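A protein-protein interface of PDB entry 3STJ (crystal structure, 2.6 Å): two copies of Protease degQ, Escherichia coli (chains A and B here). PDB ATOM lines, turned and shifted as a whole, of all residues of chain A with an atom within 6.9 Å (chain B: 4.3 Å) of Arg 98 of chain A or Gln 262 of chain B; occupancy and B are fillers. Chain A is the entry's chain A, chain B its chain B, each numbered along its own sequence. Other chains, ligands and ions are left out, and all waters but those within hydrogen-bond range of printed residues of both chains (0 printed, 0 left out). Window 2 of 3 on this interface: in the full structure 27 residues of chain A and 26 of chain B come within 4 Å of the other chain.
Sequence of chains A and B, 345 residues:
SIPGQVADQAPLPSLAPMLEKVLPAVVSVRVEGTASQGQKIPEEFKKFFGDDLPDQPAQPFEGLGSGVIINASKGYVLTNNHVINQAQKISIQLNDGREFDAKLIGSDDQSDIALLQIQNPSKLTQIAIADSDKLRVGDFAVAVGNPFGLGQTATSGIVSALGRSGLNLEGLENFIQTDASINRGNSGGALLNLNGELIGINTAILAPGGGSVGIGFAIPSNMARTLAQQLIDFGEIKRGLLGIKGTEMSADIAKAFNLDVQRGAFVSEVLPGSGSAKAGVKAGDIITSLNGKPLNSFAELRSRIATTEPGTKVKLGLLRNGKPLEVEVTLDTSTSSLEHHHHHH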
ATOM      1  N   ILE A  92      11.886  31.133   8.895  1.00  0.00           N
ATOM      2  CA  ILE A  92      11.697  31.561   7.520  1.00  0.00           C
ATOM      3  C   ILE A  92      10.954  30.455   6.775  1.00  0.00           C
ATOM      4  O   ILE A  92      11.243  29.284   6.988  1.00  0.00           O
ATOM      5  CB  ILE A  92      13.088  31.920   6.888  1.00  0.00           C
ATOM      6  CG1 ILE A  92      13.395  33.417   7.025  1.00  0.00           C
ATOM      7  CG2 ILE A  92      13.228  31.513   5.407  1.00  0.00           C
ATOM      8  CD1 ILE A  92      13.550  33.990   8.373  1.00  0.00           C
ATOM      9  N   GLN A  93       9.984  30.817   5.932  1.00  0.00           N
ATOM     10  CA  GLN A  93       9.295  29.825   5.114  1.00  0.00           C
ATOM     11  C   GLN A  93       9.425  30.220   3.657  1.00  0.00           C
ATOM     12  O   GLN A  93       9.151  31.373   3.305  1.00  0.00           O
ATOM     13  CB  GLN A  93       7.820  29.619   5.509  1.00  0.00           C
ATOM     14  CG  GLN A  93       7.219  28.435   4.754  1.00  0.00           C
ATOM     15  CD  GLN A  93       5.757  28.212   4.996  1.00  0.00           C
ATOM     16  OE1 GLN A  93       5.347  27.173   5.524  1.00  0.00           O
ATOM     17  NE2 GLN A  93       4.929  29.150   4.560  1.00  0.00           N
ATOM     18  N   LEU A  94       9.863  29.272   2.821  1.00  0.00           N
ATOM     19  CA  LEU A  94      10.011  29.474   1.383  1.00  0.00           C
ATOM     20  C   LEU A  94       8.673  29.202   0.699  1.00  0.00           C
ATOM     21  O   LEU A  94       7.809  28.544   1.281  1.00  0.00           O
ATOM     22  CB  LEU A  94      11.117  28.580   0.790  1.00  0.00           C
ATOM     23  CG  LEU A  94      12.477  28.516   1.467  1.00  0.00           C
ATOM     24  CD1 LEU A  94      13.444  27.791   0.610  1.00  0.00           C
ATOM     25  CD2 LEU A  94      13.036  29.887   1.745  1.00  0.00           C
ATOM     26  N   ASN A  95       8.500  29.684  -0.538  1.00  0.00           N
ATOM     27  CA  ASN A  95       7.244  29.484  -1.272  1.00  0.00           C
ATOM     28  C   ASN A  95       7.029  27.994  -1.698  1.00  0.00           C
ATOM     29  O   ASN A  95       5.927  27.653  -2.149  1.00  0.00           O
ATOM     30  CB  ASN A  95       7.124  30.439  -2.492  1.00  0.00           C
ATOM     31  CG  ASN A  95       8.141  30.275  -3.577  1.00  0.00           C
ATOM     32  OD1 ASN A  95       9.071  29.461  -3.506  1.00  0.00           O
ATOM     33  ND2 ASN A  95       7.980  31.056  -4.617  1.00  0.00           N
ATOM     34  N   ASP A  96       8.036  27.118  -1.510  1.00  0.00           N
ATOM     35  CA  ASP A  96       7.918  25.691  -1.808  1.00  0.00           C
ATOM     36  C   ASP A  96       7.465  24.898  -0.563  1.00  0.00           C
ATOM     37  O   ASP A  96       7.180  23.696  -0.654  1.00  0.00           O
ATOM     38  CB  ASP A  96       9.237  25.130  -2.369  1.00  0.00           C
ATOM     39  CG  ASP A  96      10.472  25.174  -1.471  1.00  0.00           C
ATOM     40  OD1 ASP A  96      10.336  25.535  -0.269  1.00  0.00           O
ATOM     41  OD2 ASP A  96      11.570  24.816  -1.962  1.00  0.00           O
ATOM     42  N   GLY A  97       7.407  25.590   0.577  1.00  0.00           N
ATOM     43  CA  GLY A  97       6.983  25.017   1.841  1.00  0.00           C
ATOM     44  C   GLY A  97       8.089  24.719   2.825  1.00  0.00           C
ATOM     45  O   GLY A  97       7.797  24.395   3.973  1.00  0.00           O
ATOM     46  N   ARG A  98       9.361  24.824   2.402  1.00  0.00           N
ATOM     47  CA  ARG A  98      10.498  24.559   3.284  1.00  0.00           C
ATOM     48  C   ARG A  98      10.620  25.619   4.364  1.00  0.00           C
ATOM     49  O   ARG A  98      10.514  26.809   4.086  1.00  0.00           O
ATOM     50  CB  ARG A  98      11.805  24.463   2.505  1.00  0.00           C
ATOM     51  CG  ARG A  98      11.931  23.197   1.702  1.00  0.00           C
ATOM     52  CD  ARG A  98      13.302  23.032   1.112  1.00  0.00           C
ATOM     53  NE  ARG A  98      13.559  23.979   0.027  1.00  0.00           N
ATOM     54  CZ  ARG A  98      14.753  24.493  -0.239  1.00  0.00           C
ATOM     55  NH1 ARG A  98      15.803  24.167   0.501  1.00  0.00           N
ATOM     56  NH2 ARG A  98      14.905  25.338  -1.248  1.00  0.00           N
ATOM     57  N   GLU A  99      10.838  25.157   5.593  1.00  0.00           N
ATOM     58  CA  GLU A  99      10.991  25.973   6.799  1.00  0.00           C
ATOM     59  C   GLU A  99      12.418  25.887   7.315  1.00  0.00           C
ATOM     60  O   GLU A  99      13.030  24.806   7.289  1.00  0.00           O
ATOM     61  CB  GLU A  99      10.003  25.522   7.898  1.00  0.00           C
ATOM     62  CG  GLU A  99       8.546  25.873   7.636  1.00  0.00           C
ATOM     63  CD  GLU A  99       7.508  24.945   8.246  1.00  0.00           C
ATOM     64  OE1 GLU A  99       7.783  24.333   9.306  1.00  0.00           O
ATOM     65  OE2 GLU A  99       6.414  24.822   7.645  1.00  0.00           O
ATOM     66  N   PHE A 100      12.940  27.018   7.785  1.00  0.00           N
ATOM     67  CA  PHE A 100      14.295  27.161   8.318  1.00  0.00           C
ATOM     68  C   PHE A 100      14.300  28.014   9.552  1.00  0.00           C
ATOM     69  O   PHE A 100      13.479  28.922   9.676  1.00  0.00           O
ATOM     70  CB  PHE A 100      15.210  27.840   7.289  1.00  0.00           C
ATOM     71  CG  PHE A 100      15.486  27.083   6.022  1.00  0.00           C
ATOM     72  CD1 PHE A 100      14.670  27.236   4.908  1.00  0.00           C
ATOM     73  CD2 PHE A 100      16.597  26.252   5.918  1.00  0.00           C
ATOM     74  CE1 PHE A 100      14.935  26.534   3.732  1.00  0.00           C
ATOM     75  CE2 PHE A 100      16.871  25.571   4.733  1.00  0.00           C
ATOM     76  CZ  PHE A 100      16.041  25.715   3.648  1.00  0.00           C
ATOM     77  N   PRO A 121      21.329  26.806   5.560  1.00  0.00           N
ATOM     78  CA  PRO A 121      20.660  27.073   4.274  1.00  0.00           C
ATOM     79  C   PRO A 121      20.973  25.994   3.244  1.00  0.00           C
ATOM     80  O   PRO A 121      22.020  25.367   3.315  1.00  0.00           O
ATOM     81  CB  PRO A 121      21.234  28.430   3.851  1.00  0.00           C
ATOM     82  CG  PRO A 121      22.533  28.530   4.526  1.00  0.00           C
ATOM     83  CD  PRO A 121      22.395  27.801   5.817  1.00  0.00           C
ATOM     84  N   SER A 122      20.058  25.767   2.304  1.00  0.00           N
ATOM     85  CA  SER A 122      20.194  24.737   1.268  1.00  0.00           C
ATOM     86  C   SER A 122      19.281  25.075   0.086  1.00  0.00           C
ATOM     87  O   SER A 122      18.127  25.428   0.303  1.00  0.00           O
ATOM     88  CB  SER A 122      19.847  23.362   1.861  1.00  0.00           C
ATOM     89  OG  SER A 122      19.444  22.377   0.923  1.00  0.00           O
ATOM     90  N   LYS A 123      19.802  24.963  -1.151  1.00  0.00           N
ATOM     91  CA  LYS A 123      19.102  25.172  -2.426  1.00  0.00           C
ATOM     92  C   LYS A 123      18.187  26.445  -2.393  1.00  0.00           C
ATOM     93  O   LYS A 123      16.994  26.389  -2.692  1.00  0.00           O
ATOM     94  CB  LYS A 123      18.289  23.911  -2.786  1.00  0.00           C
ATOM     95  CG  LYS A 123      19.114  22.677  -3.136  1.00  0.00           C
ATOM     96  CD  LYS A 123      18.206  21.476  -3.258  1.00  0.00           C
ATOM     97  CE  LYS A 123      18.877  20.228  -3.795  1.00  0.00           C
ATOM     98  NZ  LYS A 123      17.882  19.134  -4.049  1.00  0.00           N
ATOM     99  N   LEU A 124      18.782  27.582  -2.019  1.00  0.00           N
ATOM    100  CA  LEU A 124      18.155  28.891  -1.913  1.00  0.00           C
ATOM    101  C   LEU A 124      18.343  29.681  -3.212  1.00  0.00           C
ATOM    102  O   LEU A 124      19.293  29.424  -3.955  1.00  0.00           O
ATOM    103  CB  LEU A 124      18.822  29.631  -0.756  1.00  0.00           C
ATOM    104  CG  LEU A 124      18.121  29.749   0.593  1.00  0.00           C
ATOM    105  CD1 LEU A 124      17.359  28.477   1.028  1.00  0.00           C
ATOM    106  CD2 LEU A 124      19.085  30.201   1.640  1.00  0.00           C
ATOM    107  N   THR A 125      17.432  30.636  -3.492  1.00  0.00           N
ATOM    108  CA  THR A 125      17.447  31.514  -4.655  1.00  0.00           C
ATOM    109  C   THR A 125      17.629  32.931  -4.127  1.00  0.00           C
ATOM    110  O   THR A 125      16.942  33.330  -3.186  1.00  0.00           O
ATOM    111  CB  THR A 125      16.160  31.313  -5.457  1.00  0.00           C
ATOM    112  OG1 THR A 125      16.151  29.978  -5.956  1.00  0.00           O
ATOM    113  CG2 THR A 125      16.011  32.297  -6.631  1.00  0.00           C
ATOM    114  N   MET B 249       0.521  17.772   4.377  1.00  0.00           N
ATOM    115  CA  MET B 249       1.908  17.407   4.256  1.00  0.00           C
ATOM    116  C   MET B 249       2.703  18.640   4.731  1.00  0.00           C
ATOM    117  O   MET B 249       2.313  19.779   4.434  1.00  0.00           O
ATOM    118  CB  MET B 249       2.197  16.998   2.798  1.00  0.00           C
ATOM    119  CG  MET B 249       3.647  16.759   2.448  1.00  0.00           C
ATOM    120  SD  MET B 249       4.633  15.703   3.515  1.00  0.00           S
ATOM    121  CE  MET B 249       3.495  14.536   3.982  1.00  0.00           C
ATOM    122  N   SER B 250       3.757  18.415   5.526  1.00  0.00           N
ATOM    123  CA  SER B 250       4.572  19.489   6.065  1.00  0.00           C
ATOM    124  C   SER B 250       6.041  19.276   5.770  1.00  0.00           C
ATOM    125  O   SER B 250       6.449  18.186   5.386  1.00  0.00           O
ATOM    126  CB  SER B 250       4.348  19.611   7.571  1.00  0.00           C
ATOM    127  OG  SER B 250       4.764  18.460   8.289  1.00  0.00           O
ATOM    128  N   ALA B 251       6.837  20.323   5.996  1.00  0.00           N
ATOM    129  CA  ALA B 251       8.296  20.325   5.867  1.00  0.00           C
ATOM    130  C   ALA B 251       8.909  19.351   6.870  1.00  0.00           C
ATOM    131  O   ALA B 251       9.965  18.774   6.612  1.00  0.00           O
ATOM    132  CB  ALA B 251       8.830  21.733   6.092  1.00  0.00           C
ATOM    133  N   ALA B 254       8.440  15.805   5.546  1.00  0.00           N
ATOM    134  CA  ALA B 254       9.412  15.755   4.455  1.00  0.00           C
ATOM    135  C   ALA B 254      10.845  15.557   4.981  1.00  0.00           C
ATOM    136  O   ALA B 254      11.527  14.674   4.460  1.00  0.00           O
ATOM    137  CB  ALA B 254       9.325  17.015   3.621  1.00  0.00           C
ATOM    138  N   ASP B 260      11.732  15.506  -1.105  1.00  0.00           N
ATOM    139  CA  ASP B 260      11.936  16.791  -1.783  1.00  0.00           C
ATOM    140  C   ASP B 260      10.606  17.551  -2.070  1.00  0.00           C
ATOM    141  O   ASP B 260      10.598  18.542  -2.794  1.00  0.00           O
ATOM    142  CB  ASP B 260      12.750  16.585  -3.071  1.00  0.00           C
ATOM    143  CG  ASP B 260      14.232  16.420  -2.777  1.00  0.00           C
ATOM    144  OD1 ASP B 260      15.003  17.407  -2.995  1.00  0.00           O
ATOM    145  OD2 ASP B 260      14.623  15.329  -2.270  1.00  0.00           O
ATOM    146  N   VAL B 261       9.514  17.119  -1.459  1.00  0.00           N
ATOM    147  CA  VAL B 261       8.197  17.745  -1.566  1.00  0.00           C
ATOM    148  C   VAL B 261       7.685  17.981  -0.126  1.00  0.00           C
ATOM    149  O   VAL B 261       7.876  17.136   0.738  1.00  0.00           O
ATOM    150  CB  VAL B 261       7.211  16.908  -2.451  1.00  0.00           C
ATOM    151  CG1 VAL B 261       6.935  15.527  -1.853  1.00  0.00           C
ATOM    152  CG2 VAL B 261       5.903  17.662  -2.707  1.00  0.00           C
ATOM    153  N   GLN B 262       7.075  19.137   0.138  1.00  0.00           N
ATOM    154  CA  GLN B 262       6.598  19.461   1.492  1.00  0.00           C
ATOM    155  C   GLN B 262       5.156  19.933   1.480  1.00  0.00           C
ATOM    156  O   GLN B 262       4.624  20.285   2.521  1.00  0.00           O
ATOM    157  CB  GLN B 262       7.503  20.501   2.209  1.00  0.00           C
ATOM    158  CG  GLN B 262       8.355  21.412   1.312  1.00  0.00           C
ATOM    159  CD  GLN B 262       9.590  20.768   0.736  1.00  0.00           C
ATOM    160  OE1 GLN B 262       9.877  20.914  -0.447  1.00  0.00           O
ATOM    161  NE2 GLN B 262      10.378  20.087   1.552  1.00  0.00           N
ATOM    162  N   ARG B 263       4.510  19.895   0.314  1.00  0.00           N
ATOM    163  CA  ARG B 263       3.115  20.303   0.146  1.00  0.00           C
ATOM    164  C   ARG B 263       2.325  19.152  -0.491  1.00  0.00           C
ATOM    165  O   ARG B 263       2.813  18.469  -1.389  1.00  0.00           O
ATOM    166  CB  ARG B 263       3.010  21.589  -0.698  1.00  0.00           C
ATOM    167  CG  ARG B 263       3.722  22.773  -0.073  1.00  0.00           C
ATOM    168  CD  ARG B 263       3.231  24.093  -0.576  1.00  0.00           C
ATOM    169  NE  ARG B 263       3.583  24.305  -1.972  1.00  0.00           N
ATOM    170  CZ  ARG B 263       3.535  25.492  -2.564  1.00  0.00           C
ATOM    171  NH1 ARG B 263       3.159  26.569  -1.881  1.00  0.00           N
ATOM    172  NH2 ARG B 263       3.877  25.615  -3.840  1.00  0.00           N
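NH1 of Arg 263 of chain B sits at hydrogen-bond distance from O of Asn 95 of chain A (3.0 Å). The side-chain carboxylate (OD1) of Asp 260 of chain B lies within salt-bridge range of the side-chain amino group (NZ) of Lys 123 of chain A, at 3.5 Å.
NH1 of Arg 98 of chain A sits at hydrogen-bond distance from O of Ser 122 of chain A (2.7 Å). OE1 of Gln 262 of chain B sits close to O of Asp 260 of chain B. The side-chain carboxylate (OD2) of Asp 96 of chain A lies within salt-bridge range of the guanidinium group (NE) of Arg 98 of chain A (2.9 Å). NH2 of Arg 98 of chain A is in hydrogen-bond range of O of Lys 123 of chain A (2.7 Å).
Among the printed residues, pairs that only touch across the chains: Asp 96 of chain A with Gln 262 of chain B (3.2 Å), Asp 96 of chain A with Arg 263 of chain B (3.6 Å), Gly 97 of chain A with Ala 251 of chain B (3.6 Å), Gly 97 of chain A with Gln 262 of chain B (3.6 Å) and Arg 98 of chain A with Gln 262 of chain B (3.5 Å).
Of the printed residues of chain B, Asn 95 of chain A touches Arg 263. Of the printed residues of chain B, Asp 96 of chain A touches Gln 262 (3.2 Å) and Arg 263 (3.6 Å). Of the printed residues of chain B, Gly 97 of chain A touches Ala 251 (3.6 Å) and Gln 262 (3.6 Å). Arg 98 of chain A touches one residue of chain B. Of the printed residues of chain B, Lys 123 of chain A touches Asp 260 (3.5 Å). Met 249 of chain B touches none of the printed residues of chain A. Ser 250 of chain B touches none of the printed residues of chain A. Printed residues of chain A within 4 Å of Gln 262 of chain B: Asp 96 (3.2 Å), Gly 97 (3.6 Å) and Arg 98 (3.5 Å). Printed residues of chain A within 4 Å of Arg 263 of chain B: Asn 95 and Asp 96. The nearest printed residue of chain B that does not touch Arg 98 of chain A is Ala 251 of chain B (4.3 Å).
Hydrophobic or aromatic side chains of chain B within 4 Å of the printed part of chain A: Ala 251. Of the 14 printed residues of chain A, 5 touch a printed residue of chain B. Among the printed residues, Asp or Glu carboxylates within 4 Å of a Lys or Arg side-chain nitrogen of the other chain: Lys 123 of chain A with Asp 260 of chain B.
No position is printed for both chains.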
